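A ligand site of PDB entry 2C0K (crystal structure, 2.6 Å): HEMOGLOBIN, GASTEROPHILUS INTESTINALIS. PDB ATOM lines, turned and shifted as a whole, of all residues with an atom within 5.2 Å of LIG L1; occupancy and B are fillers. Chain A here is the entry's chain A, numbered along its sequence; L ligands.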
ATOM      1  N   TYR A  31     -20.397 -30.222  12.029  1.00  0.00           N
ATOM      2  CA  TYR A  31     -19.483 -29.123  11.872  1.00  0.00           C
ATOM      3  C   TYR A  31     -19.208 -28.419  13.223  1.00  0.00           C
ATOM      4  O   TYR A  31     -18.056 -28.130  13.561  1.00  0.00           O
ATOM      5  CB  TYR A  31     -20.041 -28.145  10.849  1.00  0.00           C
ATOM      6  CG  TYR A  31     -19.223 -26.906  10.611  1.00  0.00           C
ATOM      7  CD1 TYR A  31     -17.935 -26.986  10.078  1.00  0.00           C
ATOM      8  CD2 TYR A  31     -19.784 -25.620  10.812  1.00  0.00           C
ATOM      9  CE1 TYR A  31     -17.194 -25.821   9.784  1.00  0.00           C
ATOM     10  CE2 TYR A  31     -19.047 -24.456  10.532  1.00  0.00           C
ATOM     11  CZ  TYR A  31     -17.764 -24.564   9.997  1.00  0.00           C
ATOM     12  OH  TYR A  31     -17.058 -23.428   9.688  1.00  0.00           O
ATOM     13  N   ASN A  38     -16.061 -22.401  15.529  1.00  0.00           N
ATOM     14  CA  ASN A  38     -16.849 -21.742  14.471  1.00  0.00           C
ATOM     15  C   ASN A  38     -18.245 -21.303  14.952  1.00  0.00           C
ATOM     16  O   ASN A  38     -18.956 -20.572  14.254  1.00  0.00           O
ATOM     17  CB  ASN A  38     -16.985 -22.671  13.253  1.00  0.00           C
ATOM     18  CG  ASN A  38     -15.667 -22.853  12.500  1.00  0.00           C
ATOM     19  OD1 ASN A  38     -15.179 -23.979  12.312  1.00  0.00           O
ATOM     20  ND2 ASN A  38     -15.101 -21.751  12.041  1.00  0.00           N
ATOM     21  N   HIS A  41     -19.125 -17.436  15.334  1.00  0.00           N
ATOM     22  CA  HIS A  41     -19.596 -16.651  14.207  1.00  0.00           C
ATOM     23  C   HIS A  41     -21.086 -16.619  14.176  1.00  0.00           C
ATOM     24  O   HIS A  41     -21.685 -15.803  13.484  1.00  0.00           O
ATOM     25  CB  HIS A  41     -19.070 -17.227  12.882  1.00  0.00           C
ATOM     26  CG  HIS A  41     -17.627 -16.936  12.621  1.00  0.00           C
ATOM     27  ND1 HIS A  41     -17.187 -15.701  12.198  1.00  0.00           N
ATOM     28  CD2 HIS A  41     -16.520 -17.704  12.774  1.00  0.00           C
ATOM     29  CE1 HIS A  41     -15.879 -15.722  12.076  1.00  0.00           C
ATOM     30  NE2 HIS A  41     -15.440 -16.919  12.421  1.00  0.00           N
ATOM     31  N   PHE A  42     -21.693 -17.548  14.925  1.00  0.00           N
ATOM     32  CA  PHE A  42     -23.144 -17.660  14.989  1.00  0.00           C
ATOM     33  C   PHE A  42     -23.637 -17.503  16.449  1.00  0.00           C
ATOM     34  O   PHE A  42     -24.116 -18.480  17.055  1.00  0.00           O
ATOM     35  CB  PHE A  42     -23.599 -19.040  14.462  1.00  0.00           C
ATOM     36  CG  PHE A  42     -23.167 -19.324  13.052  1.00  0.00           C
ATOM     37  CD1 PHE A  42     -21.910 -19.869  12.791  1.00  0.00           C
ATOM     38  CD2 PHE A  42     -24.050 -19.173  12.003  1.00  0.00           C
ATOM     39  CE1 PHE A  42     -21.530 -20.171  11.491  1.00  0.00           C
ATOM     40  CE2 PHE A  42     -23.659 -19.491  10.691  1.00  0.00           C
ATOM     41  CZ  PHE A  42     -22.404 -19.978  10.445  1.00  0.00           C
ATOM     42  N   TRP A  44     -26.248 -16.473  17.987  1.00  0.00           N
ATOM     43  CA  TRP A  44     -27.583 -16.999  18.280  1.00  0.00           C
ATOM     44  C   TRP A  44     -27.601 -18.521  18.520  1.00  0.00           C
ATOM     45  O   TRP A  44     -28.448 -19.023  19.258  1.00  0.00           O
ATOM     46  CB  TRP A  44     -28.571 -16.634  17.165  1.00  0.00           C
ATOM     47  CG  TRP A  44     -28.003 -16.730  15.759  1.00  0.00           C
ATOM     48  CD1 TRP A  44     -28.220 -17.740  14.848  1.00  0.00           C
ATOM     49  CD2 TRP A  44     -27.140 -15.781  15.108  1.00  0.00           C
ATOM     50  NE1 TRP A  44     -27.545 -17.474  13.682  1.00  0.00           N
ATOM     51  CE2 TRP A  44     -26.876 -16.282  13.801  1.00  0.00           C
ATOM     52  CE3 TRP A  44     -26.560 -14.564  15.489  1.00  0.00           C
ATOM     53  CZ2 TRP A  44     -26.072 -15.595  12.886  1.00  0.00           C
ATOM     54  CZ3 TRP A  44     -25.753 -13.876  14.561  1.00  0.00           C
ATOM     55  CH2 TRP A  44     -25.511 -14.404  13.277  1.00  0.00           C
ATOM     56  N   ARG A  58     -34.478 -21.770  12.970  1.00  0.00           N
ATOM     57  CA  ARG A  58     -33.477 -20.979  12.294  1.00  0.00           C
ATOM     58  C   ARG A  58     -32.292 -21.855  11.889  1.00  0.00           C
ATOM     59  O   ARG A  58     -31.550 -21.552  10.965  1.00  0.00           O
ATOM     60  CB  ARG A  58     -33.021 -19.845  13.204  1.00  0.00           C
ATOM     61  CG  ARG A  58     -31.943 -18.982  12.626  1.00  0.00           C
ATOM     62  CD  ARG A  58     -31.585 -17.850  13.549  1.00  0.00           C
ATOM     63  NE  ARG A  58     -30.841 -16.809  12.863  1.00  0.00           N
ATOM     64  CZ  ARG A  58     -30.515 -15.641  13.379  1.00  0.00           C
ATOM     65  NH1 ARG A  58     -30.876 -15.348  14.632  1.00  0.00           N
ATOM     66  NH2 ARG A  58     -29.834 -14.766  12.669  1.00  0.00           N
ATOM     67  N   HIS A  62     -31.189 -22.559   8.034  1.00  0.00           N
ATOM     68  CA  HIS A  62     -29.880 -22.079   7.632  1.00  0.00           C
ATOM     69  C   HIS A  62     -29.058 -23.182   6.950  1.00  0.00           C
ATOM     70  O   HIS A  62     -28.363 -22.916   5.963  1.00  0.00           O
ATOM     71  CB  HIS A  62     -29.110 -21.519   8.804  1.00  0.00           C
ATOM     72  CG  HIS A  62     -27.821 -20.906   8.428  1.00  0.00           C
ATOM     73  ND1 HIS A  62     -27.734 -19.813   7.590  1.00  0.00           N
ATOM     74  CD2 HIS A  62     -26.548 -21.275   8.703  1.00  0.00           C
ATOM     75  CE1 HIS A  62     -26.453 -19.506   7.407  1.00  0.00           C
ATOM     76  NE2 HIS A  62     -25.714 -20.373   8.081  1.00  0.00           N
ATOM     77  N   ARG A  65     -30.276 -23.410   3.389  1.00  0.00           N
ATOM     78  CA  ARG A  65     -29.810 -22.309   2.556  1.00  0.00           C
ATOM     79  C   ARG A  65     -28.332 -22.448   2.096  1.00  0.00           C
ATOM     80  O   ARG A  65     -27.995 -22.065   1.002  1.00  0.00           O
ATOM     81  CB  ARG A  65     -30.043 -20.945   3.215  1.00  0.00           C
ATOM     82  CG  ARG A  65     -31.506 -20.606   3.403  1.00  0.00           C
ATOM     83  CD  ARG A  65     -31.862 -19.292   2.729  1.00  0.00           C
ATOM     84  NE  ARG A  65     -33.133 -18.744   3.234  1.00  0.00           N
ATOM     85  CZ  ARG A  65     -33.236 -17.959   4.306  1.00  0.00           C
ATOM     86  NH1 ARG A  65     -32.149 -17.619   5.006  1.00  0.00           N
ATOM     87  NH2 ARG A  65     -34.425 -17.507   4.684  1.00  0.00           N
ATOM     88  N   ILE A  66     -27.449 -22.966   2.982  1.00  0.00           N
ATOM     89  CA  ILE A  66     -26.038 -23.252   2.578  1.00  0.00           C
ATOM     90  C   ILE A  66     -26.003 -24.233   1.387  1.00  0.00           C
ATOM     91  O   ILE A  66     -25.345 -23.980   0.369  1.00  0.00           O
ATOM     92  CB  ILE A  66     -25.189 -23.838   3.761  1.00  0.00           C
ATOM     93  CG1 ILE A  66     -25.098 -22.816   4.903  1.00  0.00           C
ATOM     94  CG2 ILE A  66     -23.795 -24.196   3.273  1.00  0.00           C
ATOM     95  CD1 ILE A  66     -24.198 -23.237   6.070  1.00  0.00           C
ATOM     96  N   GLN A  69     -27.434 -22.935  -2.149  1.00  0.00           N
ATOM     97  CA  GLN A  69     -26.418 -22.187  -2.881  1.00  0.00           C
ATOM     98  C   GLN A  69     -25.341 -23.101  -3.486  1.00  0.00           C
ATOM     99  O   GLN A  69     -24.965 -22.926  -4.631  1.00  0.00           O
ATOM    100  CB  GLN A  69     -25.781 -21.103  -2.029  1.00  0.00           C
ATOM    101  CG  GLN A  69     -24.558 -20.498  -2.661  1.00  0.00           C
ATOM    102  CD  GLN A  69     -24.352 -19.035  -2.289  1.00  0.00           C
ATOM    103  OE1 GLN A  69     -23.954 -18.225  -3.111  1.00  0.00           O
ATOM    104  NE2 GLN A  69     -24.585 -18.705  -1.011  1.00  0.00           N
ATOM    105  N   VAL A  70     -24.891 -24.093  -2.730  1.00  0.00           N
ATOM    106  CA  VAL A  70     -24.024 -25.146  -3.292  1.00  0.00           C
ATOM    107  C   VAL A  70     -24.690 -25.796  -4.541  1.00  0.00           C
ATOM    108  O   VAL A  70     -24.010 -26.047  -5.550  1.00  0.00           O
ATOM    109  CB  VAL A  70     -23.682 -26.262  -2.243  1.00  0.00           C
ATOM    110  CG1 VAL A  70     -23.029 -27.474  -2.937  1.00  0.00           C
ATOM    111  CG2 VAL A  70     -22.787 -25.709  -1.157  1.00  0.00           C
ATOM    112  N   TRP A  90     -20.320 -17.625  -6.653  1.00  0.00           N
ATOM    113  CA  TRP A  90     -19.363 -17.488  -5.600  1.00  0.00           C
ATOM    114  C   TRP A  90     -18.910 -16.071  -5.466  1.00  0.00           C
ATOM    115  O   TRP A  90     -18.353 -15.682  -4.442  1.00  0.00           O
ATOM    116  CB  TRP A  90     -18.175 -18.440  -5.822  1.00  0.00           C
ATOM    117  CG  TRP A  90     -18.602 -19.834  -6.087  1.00  0.00           C
ATOM    118  CD1 TRP A  90     -18.478 -20.508  -7.277  1.00  0.00           C
ATOM    119  CD2 TRP A  90     -19.304 -20.707  -5.200  1.00  0.00           C
ATOM    120  NE1 TRP A  90     -19.028 -21.766  -7.163  1.00  0.00           N
ATOM    121  CE2 TRP A  90     -19.533 -21.914  -5.897  1.00  0.00           C
ATOM    122  CE3 TRP A  90     -19.735 -20.599  -3.871  1.00  0.00           C
ATOM    123  CZ2 TRP A  90     -20.192 -23.011  -5.307  1.00  0.00           C
ATOM    124  CZ3 TRP A  90     -20.376 -21.693  -3.269  1.00  0.00           C
ATOM    125  CH2 TRP A  90     -20.595 -22.886  -3.992  1.00  0.00           C
ATOM    126  N   LEU A  93     -21.499 -15.169  -2.913  1.00  0.00           N
ATOM    127  CA  LEU A  93     -21.018 -15.477  -1.562  1.00  0.00           C
ATOM    128  C   LEU A  93     -20.057 -14.368  -1.069  1.00  0.00           C
ATOM    129  O   LEU A  93     -20.196 -13.875   0.058  1.00  0.00           O
ATOM    130  CB  LEU A  93     -20.322 -16.848  -1.528  1.00  0.00           C
ATOM    131  CG  LEU A  93     -19.749 -17.320  -0.185  1.00  0.00           C
ATOM    132  CD1 LEU A  93     -20.789 -18.114   0.562  1.00  0.00           C
ATOM    133  CD2 LEU A  93     -18.478 -18.160  -0.387  1.00  0.00           C
ATOM    134  N   THR A  96     -21.886 -11.492   0.372  1.00  0.00           N
ATOM    135  CA  THR A  96     -22.730 -11.836   1.512  1.00  0.00           C
ATOM    136  C   THR A  96     -21.879 -12.087   2.778  1.00  0.00           C
ATOM    137  O   THR A  96     -22.352 -11.865   3.902  1.00  0.00           O
ATOM    138  CB  THR A  96     -23.624 -13.064   1.201  1.00  0.00           C
ATOM    139  OG1 THR A  96     -24.831 -12.624   0.586  1.00  0.00           O
ATOM    140  CG2 THR A  96     -23.956 -13.826   2.447  1.00  0.00           C
ATOM    141  N   HIS A  97     -20.635 -12.524   2.580  1.00  0.00           N
ATOM    142  CA  HIS A  97     -19.800 -13.016   3.687  1.00  0.00           C
ATOM    143  C   HIS A  97     -18.658 -12.059   4.027  1.00  0.00           C
ATOM    144  O   HIS A  97     -18.044 -12.183   5.083  1.00  0.00           O
ATOM    145  CB  HIS A  97     -19.261 -14.421   3.378  1.00  0.00           C
ATOM    146  CG  HIS A  97     -20.243 -15.512   3.650  1.00  0.00           C
ATOM    147  ND1 HIS A  97     -21.402 -15.683   2.926  1.00  0.00           N
ATOM    148  CD2 HIS A  97     -20.258 -16.482   4.608  1.00  0.00           C
ATOM    149  CE1 HIS A  97     -22.071 -16.720   3.390  1.00  0.00           C
ATOM    150  NE2 HIS A  97     -21.396 -17.224   4.408  1.00  0.00           N
ATOM    151  N   VAL A 102     -14.627 -13.965   8.528  1.00  0.00           N
ATOM    152  CA  VAL A 102     -14.429 -15.397   8.566  1.00  0.00           C
ATOM    153  C   VAL A 102     -13.215 -15.735   7.750  1.00  0.00           C
ATOM    154  O   VAL A 102     -13.133 -15.375   6.602  1.00  0.00           O
ATOM    155  CB  VAL A 102     -15.648 -16.165   7.976  1.00  0.00           C
ATOM    156  CG1 VAL A 102     -15.393 -17.661   8.020  1.00  0.00           C
ATOM    157  CG2 VAL A 102     -16.948 -15.799   8.734  1.00  0.00           C
ATOM    158  N   SER A 106     -11.833 -21.632   8.130  1.00  0.00           N
ATOM    159  CA  SER A 106     -13.202 -21.948   8.540  1.00  0.00           C
ATOM    160  C   SER A 106     -14.016 -22.543   7.387  1.00  0.00           C
ATOM    161  O   SER A 106     -14.872 -23.418   7.596  1.00  0.00           O
ATOM    162  CB  SER A 106     -13.899 -20.689   9.064  1.00  0.00           C
ATOM    163  OG  SER A 106     -13.592 -20.455  10.420  1.00  0.00           O
ATOM    164  N   TYR A 107     -13.762 -22.056   6.164  1.00  0.00           N
ATOM    165  CA  TYR A 107     -14.409 -22.561   4.972  1.00  0.00           C
ATOM    166  C   TYR A 107     -13.883 -23.946   4.602  1.00  0.00           C
ATOM    167  O   TYR A 107     -14.636 -24.819   4.167  1.00  0.00           O
ATOM    168  CB  TYR A 107     -14.190 -21.607   3.802  1.00  0.00           C
ATOM    169  CG  TYR A 107     -14.868 -20.257   3.938  1.00  0.00           C
ATOM    170  CD1 TYR A 107     -14.215 -19.193   4.576  1.00  0.00           C
ATOM    171  CD2 TYR A 107     -16.119 -20.029   3.399  1.00  0.00           C
ATOM    172  CE1 TYR A 107     -14.799 -17.954   4.655  1.00  0.00           C
ATOM    173  CE2 TYR A 107     -16.713 -18.788   3.475  1.00  0.00           C
ATOM    174  CZ  TYR A 107     -16.053 -17.746   4.107  1.00  0.00           C
ATOM    175  OH  TYR A 107     -16.637 -16.521   4.171  1.00  0.00           O
ATOM    176  N   LEU A 110     -15.488 -26.640   6.728  1.00  0.00           N
ATOM    177  CA  LEU A 110     -16.882 -26.932   6.302  1.00  0.00           C
ATOM    178  C   LEU A 110     -16.904 -27.847   5.061  1.00  0.00           C
ATOM    179  O   LEU A 110     -17.648 -28.825   5.013  1.00  0.00           O
ATOM    180  CB  LEU A 110     -17.672 -25.608   6.048  1.00  0.00           C
ATOM    181  CG  LEU A 110     -19.171 -25.760   5.707  1.00  0.00           C
ATOM    182  CD1 LEU A 110     -19.907 -26.485   6.784  1.00  0.00           C
ATOM    183  CD2 LEU A 110     -19.836 -24.381   5.418  1.00  0.00           C
ATOM    184  N   ILE A 114     -19.090 -31.111   4.599  1.00  0.00           N
ATOM    185  CA  ILE A 114     -20.020 -31.271   3.457  1.00  0.00           C
ATOM    186  C   ILE A 114     -19.637 -32.501   2.690  1.00  0.00           C
ATOM    187  O   ILE A 114     -20.494 -33.351   2.354  1.00  0.00           O
ATOM    188  CB  ILE A 114     -20.007 -30.075   2.494  1.00  0.00           C
ATOM    189  CG1 ILE A 114     -20.625 -28.854   3.139  1.00  0.00           C
ATOM    190  CG2 ILE A 114     -20.758 -30.423   1.220  1.00  0.00           C
ATOM    191  CD1 ILE A 114     -20.272 -27.542   2.448  1.00  0.00           C
ATOM    192  N   PHE A 136     -14.743 -27.295  -4.503  1.00  0.00           N
ATOM    193  CA  PHE A 136     -14.859 -26.343  -3.397  1.00  0.00           C
ATOM    194  C   PHE A 136     -13.643 -25.446  -3.287  1.00  0.00           C
ATOM    195  O   PHE A 136     -13.789 -24.229  -3.037  1.00  0.00           O
ATOM    196  CB  PHE A 136     -15.132 -27.049  -2.078  1.00  0.00           C
ATOM    197  CG  PHE A 136     -16.584 -27.366  -1.848  1.00  0.00           C
ATOM    198  CD1 PHE A 136     -17.486 -26.358  -1.492  1.00  0.00           C
ATOM    199  CD2 PHE A 136     -17.058 -28.664  -1.957  1.00  0.00           C
ATOM    200  CE1 PHE A 136     -18.828 -26.648  -1.257  1.00  0.00           C
ATOM    201  CE2 PHE A 136     -18.412 -28.966  -1.725  1.00  0.00           C
ATOM    202  CZ  PHE A 136     -19.282 -27.964  -1.375  1.00  0.00           C
ATOM    203  N   TYR A 140     -14.030 -21.449  -3.440  1.00  0.00           N
ATOM    204  CA  TYR A 140     -13.377 -20.641  -2.382  1.00  0.00           C
ATOM    205  C   TYR A 140     -12.319 -19.686  -2.964  1.00  0.00           C
ATOM    206  O   TYR A 140     -12.156 -18.552  -2.502  1.00  0.00           O
ATOM    207  CB  TYR A 140     -12.755 -21.549  -1.300  1.00  0.00           C
ATOM    208  CG  TYR A 140     -13.782 -22.296  -0.432  1.00  0.00           C
ATOM    209  CD1 TYR A 140     -13.414 -23.449   0.296  1.00  0.00           C
ATOM    210  CD2 TYR A 140     -15.097 -21.867  -0.339  1.00  0.00           C
ATOM    211  CE1 TYR A 140     -14.334 -24.127   1.088  1.00  0.00           C
ATOM    212  CE2 TYR A 140     -16.039 -22.554   0.447  1.00  0.00           C
ATOM    213  CZ  TYR A 140     -15.656 -23.659   1.158  1.00  0.00           C
ATOM    214  OH  TYR A 140     -16.579 -24.314   1.942  1.00  0.00           O
HETATM  215  C1  LIG L   1     -25.206 -16.427   5.815  1.00  0.00           C
HETATM  216  C2  LIG L   1     -23.990 -19.686   2.311  1.00  0.00           C
HETATM  217  C3  LIG L   1     -19.764 -20.670   4.530  1.00  0.00           C
HETATM  218  C4  LIG L   1     -21.078 -17.681   8.191  1.00  0.00           C
HETATM  219  C5  LIG L   1     -25.273 -17.261   4.702  1.00  0.00           C
HETATM  220  C6  LIG L   1     -26.440 -17.467   3.845  1.00  0.00           C
HETATM  221  C7  LIG L   1     -26.105 -18.365   2.887  1.00  0.00           C
HETATM  222  C8  LIG L   1     -24.708 -18.763   3.097  1.00  0.00           C
HETATM  223  C9  LIG L   1     -27.061 -18.860   1.758  1.00  0.00           C
HETATM  224  C10 LIG L   1     -27.836 -16.830   4.029  1.00  0.00           C
HETATM  225  C11 LIG L   1     -27.870 -15.350   3.704  1.00  0.00           C
HETATM  226  C12 LIG L   1     -29.331 -14.903   3.763  1.00  0.00           C
HETATM  227  O1  LIG L   1     -29.685 -13.933   3.029  1.00  0.00           O
HETATM  228  O2  LIG L   1     -30.133 -15.553   4.532  1.00  0.00           O
HETATM  229  C13 LIG L   1     -22.730 -20.241   2.596  1.00  0.00           C
HETATM  230  C14 LIG L   1     -21.978 -21.175   1.753  1.00  0.00           C
HETATM  231  C15 LIG L   1     -20.813 -21.455   2.381  1.00  0.00           C
HETATM  232  C16 LIG L   1     -20.778 -20.687   3.609  1.00  0.00           C
HETATM  233  C17 LIG L   1     -22.484 -21.774   0.405  1.00  0.00           C
HETATM  234  C18 LIG L   1     -19.670 -22.389   1.879  1.00  0.00           C
HETATM  235  C19 LIG L   1     -19.920 -23.614   1.432  1.00  0.00           C
HETATM  236  C20 LIG L   1     -19.786 -20.003   5.730  1.00  0.00           C
HETATM  237  C21 LIG L   1     -18.827 -20.164   6.804  1.00  0.00           C
HETATM  238  C22 LIG L   1     -19.192 -19.343   7.820  1.00  0.00           C
HETATM  239  C23 LIG L   1     -20.403 -18.639   7.423  1.00  0.00           C
HETATM  240  C24 LIG L   1     -17.626 -21.116   6.788  1.00  0.00           C
HETATM  241  C25 LIG L   1     -18.471 -19.167   9.188  1.00  0.00           C
HETATM  242  C26 LIG L   1     -18.462 -20.160  10.070  1.00  0.00           C
HETATM  243  C27 LIG L   1     -22.326 -17.117   7.952  1.00  0.00           C
HETATM  244  C28 LIG L   1     -23.117 -16.347   8.895  1.00  0.00           C
HETATM  245  C29 LIG L   1     -24.384 -15.937   8.155  1.00  0.00           C
HETATM  246  C30 LIG L   1     -24.270 -16.522   6.826  1.00  0.00           C
HETATM  247  C31 LIG L   1     -22.735 -15.983  10.364  1.00  0.00           C
HETATM  248  C32 LIG L   1     -25.573 -15.135   8.725  1.00  0.00           C
HETATM  249  C33 LIG L   1     -26.523 -16.125   9.399  1.00  0.00           C
HETATM  250  C34 LIG L   1     -27.876 -15.502   9.652  1.00  0.00           C
HETATM  251  O3  LIG L   1     -28.863 -16.274   9.801  1.00  0.00           O
HETATM  252  O4  LIG L   1     -27.967 -14.258   9.740  1.00  0.00           O
HETATM  253  N1  LIG L   1     -24.240 -18.064   4.211  1.00  0.00           N
HETATM  254  N2  LIG L   1     -21.969 -19.980   3.705  1.00  0.00           N
HETATM  255  N3  LIG L   1     -20.738 -19.067   6.140  1.00  0.00           N
HETATM  256  N4  LIG L   1     -23.045 -17.201   6.746  1.00  0.00           N
HETATM  257 FE1  LIG L   1     -22.490 -18.587   5.291  1.00  0.00          FE
HETATM  258  O1  LG2 L   2     -23.747 -19.679   6.094  1.00  0.00           O
HETATM  259  O2  LG2 L   2     -23.004 -20.479   6.595  1.00  0.00           O
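OH of Tyr 140 sits at hydrogen-bond distance from O of Tyr 107 (3.0 Å). The side-chain hydroxyl (OH) of Tyr 31 lies within hydrogen-bond range of the backbone carbonyl oxygen (O) of Ser 106 (3.0 Å). OH of Tyr 31 sits close to OD1 of Asn 38, 3.3 Å away. OG of Ser 106 is in hydrogen-bond range of ND2 of Asn 38, 2.6 Å away.
An iron atom (FE1) of LIG L1 is bound by a ring nitrogen (NE2) of His 97. NH1 of Arg 65 lies within salt-bridge range of O2 of LIG L1 (2.9 Å). The guanidinium group (NH2) of Arg 58 is in salt-bridge range of an oxygen (O3) of LIG L1 (3.4 Å). A ring nitrogen (NE2) of His 62 lies close to an oxygen (O1) of LG2 L2 (2.9 Å).
An oxygen (O1) of LG2 L2 is bound to an iron atom (FE1) of LIG L1.
Tyr 31 touches LIG L1. His 41 touches LIG L1 (O to C31, 3.3 Å). CE1 of Phe 42 touches C26 of LIG L1 (3.4 Å). Trp 44 touches LIG L1. His 62 touches LIG L1. O of Ile 66 touches C17 of LIG L1, 3.6 Å away. NE2 of Gln 69 touches C2 of LIG L1 (3.5 Å). CD1 of Leu 93 touches C14 of LIG L1, at 3.5 Å. CG1 of Val 102 touches C25 of LIG L1, 3.6 Å away. O of Ser 106 touches C24 of LIG L1 (3.7 Å). Tyr 107 touches LIG L1 (CE2 to C3, 3.7 Å). Leu 110 touches LIG L1. Tyr 140 touches LIG L1 (OH to C19, 3.5 Å). 16 residues have an atom within 4 Å of LIG L1: Tyr 31, His 41, Phe 42, Trp 44, Arg 58, His 62, Arg 65, Ile 66, Gln 69, Leu 93, His 97, Val 102, Ser 106, Tyr 107, Leu 110 and Tyr 140. The nearest printed residue that does not touch LIG L1 is Ile 114 (4.1 Å).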
